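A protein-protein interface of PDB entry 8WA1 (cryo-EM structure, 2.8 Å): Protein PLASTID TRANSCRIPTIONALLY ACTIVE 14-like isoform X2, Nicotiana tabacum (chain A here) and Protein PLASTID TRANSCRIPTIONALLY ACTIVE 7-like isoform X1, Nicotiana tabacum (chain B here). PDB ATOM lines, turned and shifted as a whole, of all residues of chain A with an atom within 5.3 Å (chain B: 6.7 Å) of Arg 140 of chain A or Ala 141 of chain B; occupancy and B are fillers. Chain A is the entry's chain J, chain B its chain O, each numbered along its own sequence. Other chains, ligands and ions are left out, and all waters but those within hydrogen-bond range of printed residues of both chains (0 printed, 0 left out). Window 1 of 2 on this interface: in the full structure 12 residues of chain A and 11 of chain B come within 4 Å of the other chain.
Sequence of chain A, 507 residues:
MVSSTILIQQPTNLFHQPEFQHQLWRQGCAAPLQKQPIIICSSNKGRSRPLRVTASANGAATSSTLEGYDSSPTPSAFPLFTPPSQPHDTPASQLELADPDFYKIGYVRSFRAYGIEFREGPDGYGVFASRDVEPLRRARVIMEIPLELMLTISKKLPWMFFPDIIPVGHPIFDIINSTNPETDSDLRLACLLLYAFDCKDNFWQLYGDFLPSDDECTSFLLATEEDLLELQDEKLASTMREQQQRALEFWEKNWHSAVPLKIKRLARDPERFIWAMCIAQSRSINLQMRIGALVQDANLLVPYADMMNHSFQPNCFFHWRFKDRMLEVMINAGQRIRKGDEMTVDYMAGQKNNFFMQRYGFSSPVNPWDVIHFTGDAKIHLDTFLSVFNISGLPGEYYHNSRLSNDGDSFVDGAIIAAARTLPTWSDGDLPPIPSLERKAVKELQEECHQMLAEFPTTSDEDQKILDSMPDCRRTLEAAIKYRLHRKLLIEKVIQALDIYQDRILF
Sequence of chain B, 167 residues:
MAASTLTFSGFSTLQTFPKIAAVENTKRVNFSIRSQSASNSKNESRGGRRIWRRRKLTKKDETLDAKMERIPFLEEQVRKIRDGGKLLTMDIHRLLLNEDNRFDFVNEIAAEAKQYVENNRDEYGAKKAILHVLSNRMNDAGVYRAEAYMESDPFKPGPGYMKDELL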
ATOM      1  N   ARG A 131       0.571  14.944  -3.295  1.00  0.00           N
ATOM      2  CA  ARG A 131      -0.475  15.935  -3.492  1.00  0.00           C
ATOM      3  C   ARG A 131      -1.812  15.211  -3.529  1.00  0.00           C
ATOM      4  O   ARG A 131      -1.908  14.071  -3.992  1.00  0.00           O
ATOM      5  CB  ARG A 131      -0.245  16.738  -4.779  1.00  0.00           C
ATOM      6  CG  ARG A 131      -1.281  17.815  -5.065  1.00  0.00           C
ATOM      7  CD  ARG A 131      -0.935  18.581  -6.333  1.00  0.00           C
ATOM      8  NE  ARG A 131      -0.798  17.695  -7.486  1.00  0.00           N
ATOM      9  CZ  ARG A 131      -0.364  18.084  -8.680  1.00  0.00           C
ATOM     10  NH1 ARG A 131      -0.018  19.348  -8.883  1.00  0.00           N
ATOM     11  NH2 ARG A 131      -0.272  17.209  -9.672  1.00  0.00           N
ATOM     12  N   VAL A 133      -5.304  14.555  -5.000  1.00  0.00           N
ATOM     13  CA  VAL A 133      -5.939  14.649  -6.309  1.00  0.00           C
ATOM     14  C   VAL A 133      -7.377  14.171  -6.188  1.00  0.00           C
ATOM     15  O   VAL A 133      -7.626  13.009  -5.843  1.00  0.00           O
ATOM     16  CB  VAL A 133      -5.176  13.833  -7.366  1.00  0.00           C
ATOM     17  CG1 VAL A 133      -5.835  13.980  -8.728  1.00  0.00           C
ATOM     18  CG2 VAL A 133      -3.720  14.263  -7.420  1.00  0.00           C
ATOM     19  N   LEU A 136     -10.851  13.214 -11.319  1.00  0.00           N
ATOM     20  CA  LEU A 136     -10.673  14.085 -12.470  1.00  0.00           C
ATOM     21  C   LEU A 136     -11.481  13.569 -13.652  1.00  0.00           C
ATOM     22  O   LEU A 136     -11.794  12.378 -13.743  1.00  0.00           O
ATOM     23  CB  LEU A 136      -9.193  14.189 -12.866  1.00  0.00           C
ATOM     24  CG  LEU A 136      -8.215  14.677 -11.796  1.00  0.00           C
ATOM     25  CD1 LEU A 136      -6.788  14.651 -12.321  1.00  0.00           C
ATOM     26  CD2 LEU A 136      -8.587  16.074 -11.321  1.00  0.00           C
ATOM     27  N   ARG A 138     -10.362  13.660 -16.759  1.00  0.00           N
ATOM     28  CA  ARG A 138      -9.404  13.007 -17.638  1.00  0.00           C
ATOM     29  C   ARG A 138      -8.131  12.692 -16.866  1.00  0.00           C
ATOM     30  O   ARG A 138      -7.913  13.182 -15.754  1.00  0.00           O
ATOM     31  CB  ARG A 138      -9.084  13.874 -18.863  1.00  0.00           C
ATOM     32  CG  ARG A 138     -10.107  13.756 -19.982  1.00  0.00           C
ATOM     33  CD  ARG A 138      -9.921  14.839 -21.030  1.00  0.00           C
ATOM     34  NE  ARG A 138     -10.433  16.128 -20.575  1.00  0.00           N
ATOM     35  CZ  ARG A 138     -11.687  16.532 -20.749  1.00  0.00           C
ATOM     36  NH1 ARG A 138     -12.558  15.747 -21.368  1.00  0.00           N
ATOM     37  NH2 ARG A 138     -12.071  17.721 -20.305  1.00  0.00           N
ATOM     38  N   ALA A 139      -7.290  11.860 -17.474  1.00  0.00           N
ATOM     39  CA  ALA A 139      -6.068  11.412 -16.820  1.00  0.00           C
ATOM     40  C   ALA A 139      -5.087  12.564 -16.639  1.00  0.00           C
ATOM     41  O   ALA A 139      -5.053  13.515 -17.427  1.00  0.00           O
ATOM     42  CB  ALA A 139      -5.416  10.294 -17.632  1.00  0.00           C
ATOM     43  N   ARG A 140      -4.283  12.473 -15.582  1.00  0.00           N
ATOM     44  CA  ARG A 140      -3.233  13.439 -15.290  1.00  0.00           C
ATOM     45  C   ARG A 140      -1.876  12.758 -15.407  1.00  0.00           C
ATOM     46  O   ARG A 140      -1.690  11.639 -14.921  1.00  0.00           O
ATOM     47  CB  ARG A 140      -3.403  14.040 -13.891  1.00  0.00           C
ATOM     48  CG  ARG A 140      -2.302  15.011 -13.495  1.00  0.00           C
ATOM     49  CD  ARG A 140      -2.533  15.582 -12.105  1.00  0.00           C
ATOM     50  NE  ARG A 140      -3.770  16.353 -12.029  1.00  0.00           N
ATOM     51  CZ  ARG A 140      -4.178  17.004 -10.945  1.00  0.00           C
ATOM     52  NH1 ARG A 140      -3.445  16.982  -9.841  1.00  0.00           N
ATOM     53  NH2 ARG A 140      -5.318  17.680 -10.966  1.00  0.00           N
ATOM     54  N   VAL A 141      -0.930  13.442 -16.043  1.00  0.00           N
ATOM     55  CA  VAL A 141       0.380  12.875 -16.342  1.00  0.00           C
ATOM     56  C   VAL A 141       1.299  13.121 -15.151  1.00  0.00           C
ATOM     57  O   VAL A 141       1.592  14.269 -14.808  1.00  0.00           O
ATOM     58  CB  VAL A 141       0.968  13.471 -17.626  1.00  0.00           C
ATOM     59  CG1 VAL A 141       2.289  12.805 -17.959  1.00  0.00           C
ATOM     60  CG2 VAL A 141      -0.015  13.329 -18.777  1.00  0.00           C
ATOM     61  N   ILE A 142       1.759  12.039 -14.518  1.00  0.00           N
ATOM     62  CA  ILE A 142       2.686  12.179 -13.400  1.00  0.00           C
ATOM     63  C   ILE A 142       4.129  12.045 -13.875  1.00  0.00           C
ATOM     64  O   ILE A 142       5.041  12.655 -13.304  1.00  0.00           O
ATOM     65  CB  ILE A 142       2.357  11.162 -12.291  1.00  0.00           C
ATOM     66  CG1 ILE A 142       2.421   9.731 -12.825  1.00  0.00           C
ATOM     67  CG2 ILE A 142       0.993  11.456 -11.692  1.00  0.00           C
ATOM     68  CD1 ILE A 142       2.194   8.679 -11.763  1.00  0.00           C
ATOM     69  N   VAL A 329       3.153   8.290 -17.862  1.00  0.00           N
ATOM     70  CA  VAL A 329       2.372   7.544 -16.884  1.00  0.00           C
ATOM     71  C   VAL A 329       1.245   8.448 -16.409  1.00  0.00           C
ATOM     72  O   VAL A 329       1.494   9.551 -15.906  1.00  0.00           O
ATOM     73  CB  VAL A 329       3.244   7.077 -15.708  1.00  0.00           C
ATOM     74  CG1 VAL A 329       2.435   6.211 -14.758  1.00  0.00           C
ATOM     75  CG2 VAL A 329       4.466   6.327 -16.217  1.00  0.00           C
ATOM     76  N   MET A 330       0.004   7.994 -16.570  1.00  0.00           N
ATOM     77  CA  MET A 330      -1.169   8.807 -16.280  1.00  0.00           C
ATOM     78  C   MET A 330      -2.054   8.106 -15.260  1.00  0.00           C
ATOM     79  O   MET A 330      -2.294   6.899 -15.364  1.00  0.00           O
ATOM     80  CB  MET A 330      -1.961   9.101 -17.556  1.00  0.00           C
ATOM     81  CG  MET A 330      -1.174   9.862 -18.608  1.00  0.00           C
ATOM     82  SD  MET A 330      -2.222  10.581 -19.886  1.00  0.00           S
ATOM     83  CE  MET A 330      -3.058   9.124 -20.500  1.00  0.00           C
ATOM     84  N   ILE A 331      -2.535   8.870 -14.279  1.00  0.00           N
ATOM     85  CA  ILE A 331      -3.450   8.339 -13.277  1.00  0.00           C
ATOM     86  C   ILE A 331      -4.790   8.032 -13.930  1.00  0.00           C
ATOM     87  O   ILE A 331      -5.246   8.761 -14.820  1.00  0.00           O
ATOM     88  CB  ILE A 331      -3.609   9.333 -12.117  1.00  0.00           C
ATOM     89  CG1 ILE A 331      -2.244   9.706 -11.542  1.00  0.00           C
ATOM     90  CG2 ILE A 331      -4.501   8.760 -11.026  1.00  0.00           C
ATOM     91  CD1 ILE A 331      -2.322  10.639 -10.355  1.00  0.00           C
ATOM     92  N   ARG B  94       0.508  22.603 -25.672  1.00  0.00           N
ATOM     93  CA  ARG B  94       0.553  21.432 -24.802  1.00  0.00           C
ATOM     94  C   ARG B  94      -0.650  20.526 -25.033  1.00  0.00           C
ATOM     95  O   ARG B  94      -0.525  19.296 -25.000  1.00  0.00           O
ATOM     96  CB  ARG B  94       0.629  21.872 -23.338  1.00  0.00           C
ATOM     97  CG  ARG B  94       1.146  20.806 -22.379  1.00  0.00           C
ATOM     98  CD  ARG B  94       0.028  19.928 -21.836  1.00  0.00           C
ATOM     99  NE  ARG B  94       0.525  18.909 -20.915  1.00  0.00           N
ATOM    100  CZ  ARG B  94       0.917  17.695 -21.285  1.00  0.00           C
ATOM    101  NH1 ARG B  94       0.873  17.342 -22.561  1.00  0.00           N
ATOM    102  NH2 ARG B  94       1.353  16.833 -20.377  1.00  0.00           N
ATOM    103  N   LEU B  95      -1.824  21.112 -25.266  1.00  0.00           N
ATOM    104  CA  LEU B  95      -3.025  20.325 -25.513  1.00  0.00           C
ATOM    105  C   LEU B  95      -3.078  19.751 -26.920  1.00  0.00           C
ATOM    106  O   LEU B  95      -3.791  18.764 -27.140  1.00  0.00           O
ATOM    107  CB  LEU B  95      -4.274  21.172 -25.259  1.00  0.00           C
ATOM    108  CG  LEU B  95      -4.536  21.601 -23.815  1.00  0.00           C
ATOM    109  CD1 LEU B  95      -5.841  22.376 -23.716  1.00  0.00           C
ATOM    110  CD2 LEU B  95      -4.555  20.394 -22.891  1.00  0.00           C
ATOM    111  N   ASN B 136     -10.042  25.069 -17.560  1.00  0.00           N
ATOM    112  CA  ASN B 136     -10.458  23.868 -16.843  1.00  0.00           C
ATOM    113  C   ASN B 136      -9.615  22.666 -17.252  1.00  0.00           C
ATOM    114  O   ASN B 136      -9.218  21.859 -16.404  1.00  0.00           O
ATOM    115  CB  ASN B 136     -11.943  23.593 -17.086  1.00  0.00           C
ATOM    116  CG  ASN B 136     -12.840  24.629 -16.436  1.00  0.00           C
ATOM    117  OD1 ASN B 136     -13.838  25.054 -17.017  1.00  0.00           O
ATOM    118  ND2 ASN B 136     -12.484  25.044 -15.227  1.00  0.00           N
ATOM    119  N   ARG B 137      -9.320  22.539 -18.549  1.00  0.00           N
ATOM    120  CA  ARG B 137      -8.506  21.418 -19.012  1.00  0.00           C
ATOM    121  C   ARG B 137      -7.074  21.527 -18.499  1.00  0.00           C
ATOM    122  O   ARG B 137      -6.425  20.513 -18.215  1.00  0.00           O
ATOM    123  CB  ARG B 137      -8.535  21.339 -20.538  1.00  0.00           C
ATOM    124  CG  ARG B 137      -9.884  20.924 -21.098  1.00  0.00           C
ATOM    125  CD  ARG B 137      -9.737  20.197 -22.423  1.00  0.00           C
ATOM    126  NE  ARG B 137     -11.025  19.726 -22.926  1.00  0.00           N
ATOM    127  CZ  ARG B 137     -11.168  18.918 -23.970  1.00  0.00           C
ATOM    128  NH1 ARG B 137     -10.101  18.482 -24.626  1.00  0.00           N
ATOM    129  NH2 ARG B 137     -12.379  18.543 -24.357  1.00  0.00           N
ATOM    130  N   MET B 138      -6.557  22.753 -18.380  1.00  0.00           N
ATOM    131  CA  MET B 138      -5.210  22.924 -17.843  1.00  0.00           C
ATOM    132  C   MET B 138      -5.172  22.663 -16.340  1.00  0.00           C
ATOM    133  O   MET B 138      -4.210  22.075 -15.833  1.00  0.00           O
ATOM    134  CB  MET B 138      -4.686  24.322 -18.163  1.00  0.00           C
ATOM    135  CG  MET B 138      -4.367  24.538 -19.634  1.00  0.00           C
ATOM    136  SD  MET B 138      -3.139  23.375 -20.262  1.00  0.00           S
ATOM    137  CE  MET B 138      -1.730  23.778 -19.233  1.00  0.00           C
ATOM    138  N   ASN B 139      -6.204  23.093 -15.611  1.00  0.00           N
ATOM    139  CA  ASN B 139      -6.238  22.866 -14.169  1.00  0.00           C
ATOM    140  C   ASN B 139      -6.429  21.390 -13.848  1.00  0.00           C
ATOM    141  O   ASN B 139      -5.885  20.890 -12.855  1.00  0.00           O
ATOM    142  CB  ASN B 139      -7.344  23.703 -13.528  1.00  0.00           C
ATOM    143  CG  ASN B 139      -7.042  25.187 -13.556  1.00  0.00           C
ATOM    144  OD1 ASN B 139      -6.217  25.648 -14.344  1.00  0.00           O
ATOM    145  ND2 ASN B 139      -7.708  25.943 -12.692  1.00  0.00           N
ATOM    146  N   ASP B 140      -7.202  20.677 -14.669  1.00  0.00           N
ATOM    147  CA  ASP B 140      -7.385  19.247 -14.467  1.00  0.00           C
ATOM    148  C   ASP B 140      -6.139  18.439 -14.806  1.00  0.00           C
ATOM    149  O   ASP B 140      -6.103  17.238 -14.517  1.00  0.00           O
ATOM    150  CB  ASP B 140      -8.570  18.747 -15.297  1.00  0.00           C
ATOM    151  CG  ASP B 140      -9.890  19.338 -14.839  1.00  0.00           C
ATOM    152  OD1 ASP B 140      -9.882  20.143 -13.883  1.00  0.00           O
ATOM    153  OD2 ASP B 140     -10.936  18.999 -15.432  1.00  0.00           O
ATOM    154  N   ALA B 141      -5.123  19.062 -15.402  1.00  0.00           N
ATOM    155  CA  ALA B 141      -3.886  18.386 -15.764  1.00  0.00           C
ATOM    156  C   ALA B 141      -2.759  18.649 -14.775  1.00  0.00           C
ATOM    157  O   ALA B 141      -1.633  18.193 -14.997  1.00  0.00           O
ATOM    158  CB  ALA B 141      -3.452  18.801 -17.171  1.00  0.00           C
ATOM    159  N   GLY B 142      -3.031  19.371 -13.689  1.00  0.00           N
ATOM    160  CA  GLY B 142      -2.031  19.660 -12.684  1.00  0.00           C
ATOM    161  C   GLY B 142      -1.357  21.009 -12.811  1.00  0.00           C
ATOM    162  O   GLY B 142      -0.496  21.328 -11.981  1.00  0.00           O
ATOM    163  N   VAL B 143      -1.717  21.809 -13.810  1.00  0.00           N
ATOM    164  CA  VAL B 143      -1.121  23.119 -14.039  1.00  0.00           C
ATOM    165  C   VAL B 143      -2.137  24.182 -13.652  1.00  0.00           C
ATOM    166  O   VAL B 143      -3.247  24.215 -14.195  1.00  0.00           O
ATOM    167  CB  VAL B 143      -0.677  23.289 -15.502  1.00  0.00           C
ATOM    168  CG1 VAL B 143       0.001  24.637 -15.698  1.00  0.00           C
ATOM    169  CG2 VAL B 143       0.245  22.155 -15.911  1.00  0.00           C
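Printed residues of chain A that touch a printed residue of chain B: Arg 131, Leu 136, Arg 138 and Arg 140. Hydrophobic or aromatic side chains of chain A that line the printed part of chain B: Leu 136. Of the 10 printed residues of chain B, 5 touch a printed residue of chain A. Among the printed residues, 7 pairs touch across the chains. Among the printed residues, no Asp or Glu carboxylate lies within 4 Å of a Lys or Arg side-chain nitrogen of the other chain.
O of Arg 140 of chain A is in hydrogen-bond range of N of Ile 331 of chain A, 3.0 Å away. O of Val 143 of chain B lies close to OD1 of Asn 139 of chain B (3.3 Å).
Arg 140 of chain A touches just these residues of chain B: Asn 139 (3.8 Å), Asp 140 (3.5 Å), Ala 141 (3.6 Å) and Gly 142 (3.5 Å). Ala 141 of chain B touches one residue of chain A. Of the printed residues of chain A, Asp 140 of chain B touches Leu 136 (3.5 Å) and Arg 140 (3.5 Å). Of the printed residues of chain A, Asn 139 of chain B touches Arg 140 (3.8 Å). Of the printed residues of chain A, Arg 137 of chain B touches Arg 138. Val 141 of chain A touches none of the printed residues of chain B. Ala 139 of chain A touches none of the printed residues of chain B. The nearest residue of chain A that does not touch Ala 141 of chain B is Val 141 of chain A (4.9 Å).
Among the printed residues, pairs that only touch across the chains: Arg 131 of chain A with Gly 142 of chain B (3.7 Å), Leu 136 of chain A with Asp 140 of chain B (3.5 Å), Arg 140 of chain A with Asn 139 of chain B (3.8 Å), Arg 140 of chain A with Asp 140 of chain B (3.5 Å), Arg 140 of chain A with Ala 141 of chain B (3.6 Å) and Arg 140 of chain A with Gly 142 of chain B (3.5 Å).
The guanidinium group of Arg 138 of chain A lies close to the guanidinium group of Arg 137 of chain B (3.5 Å).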
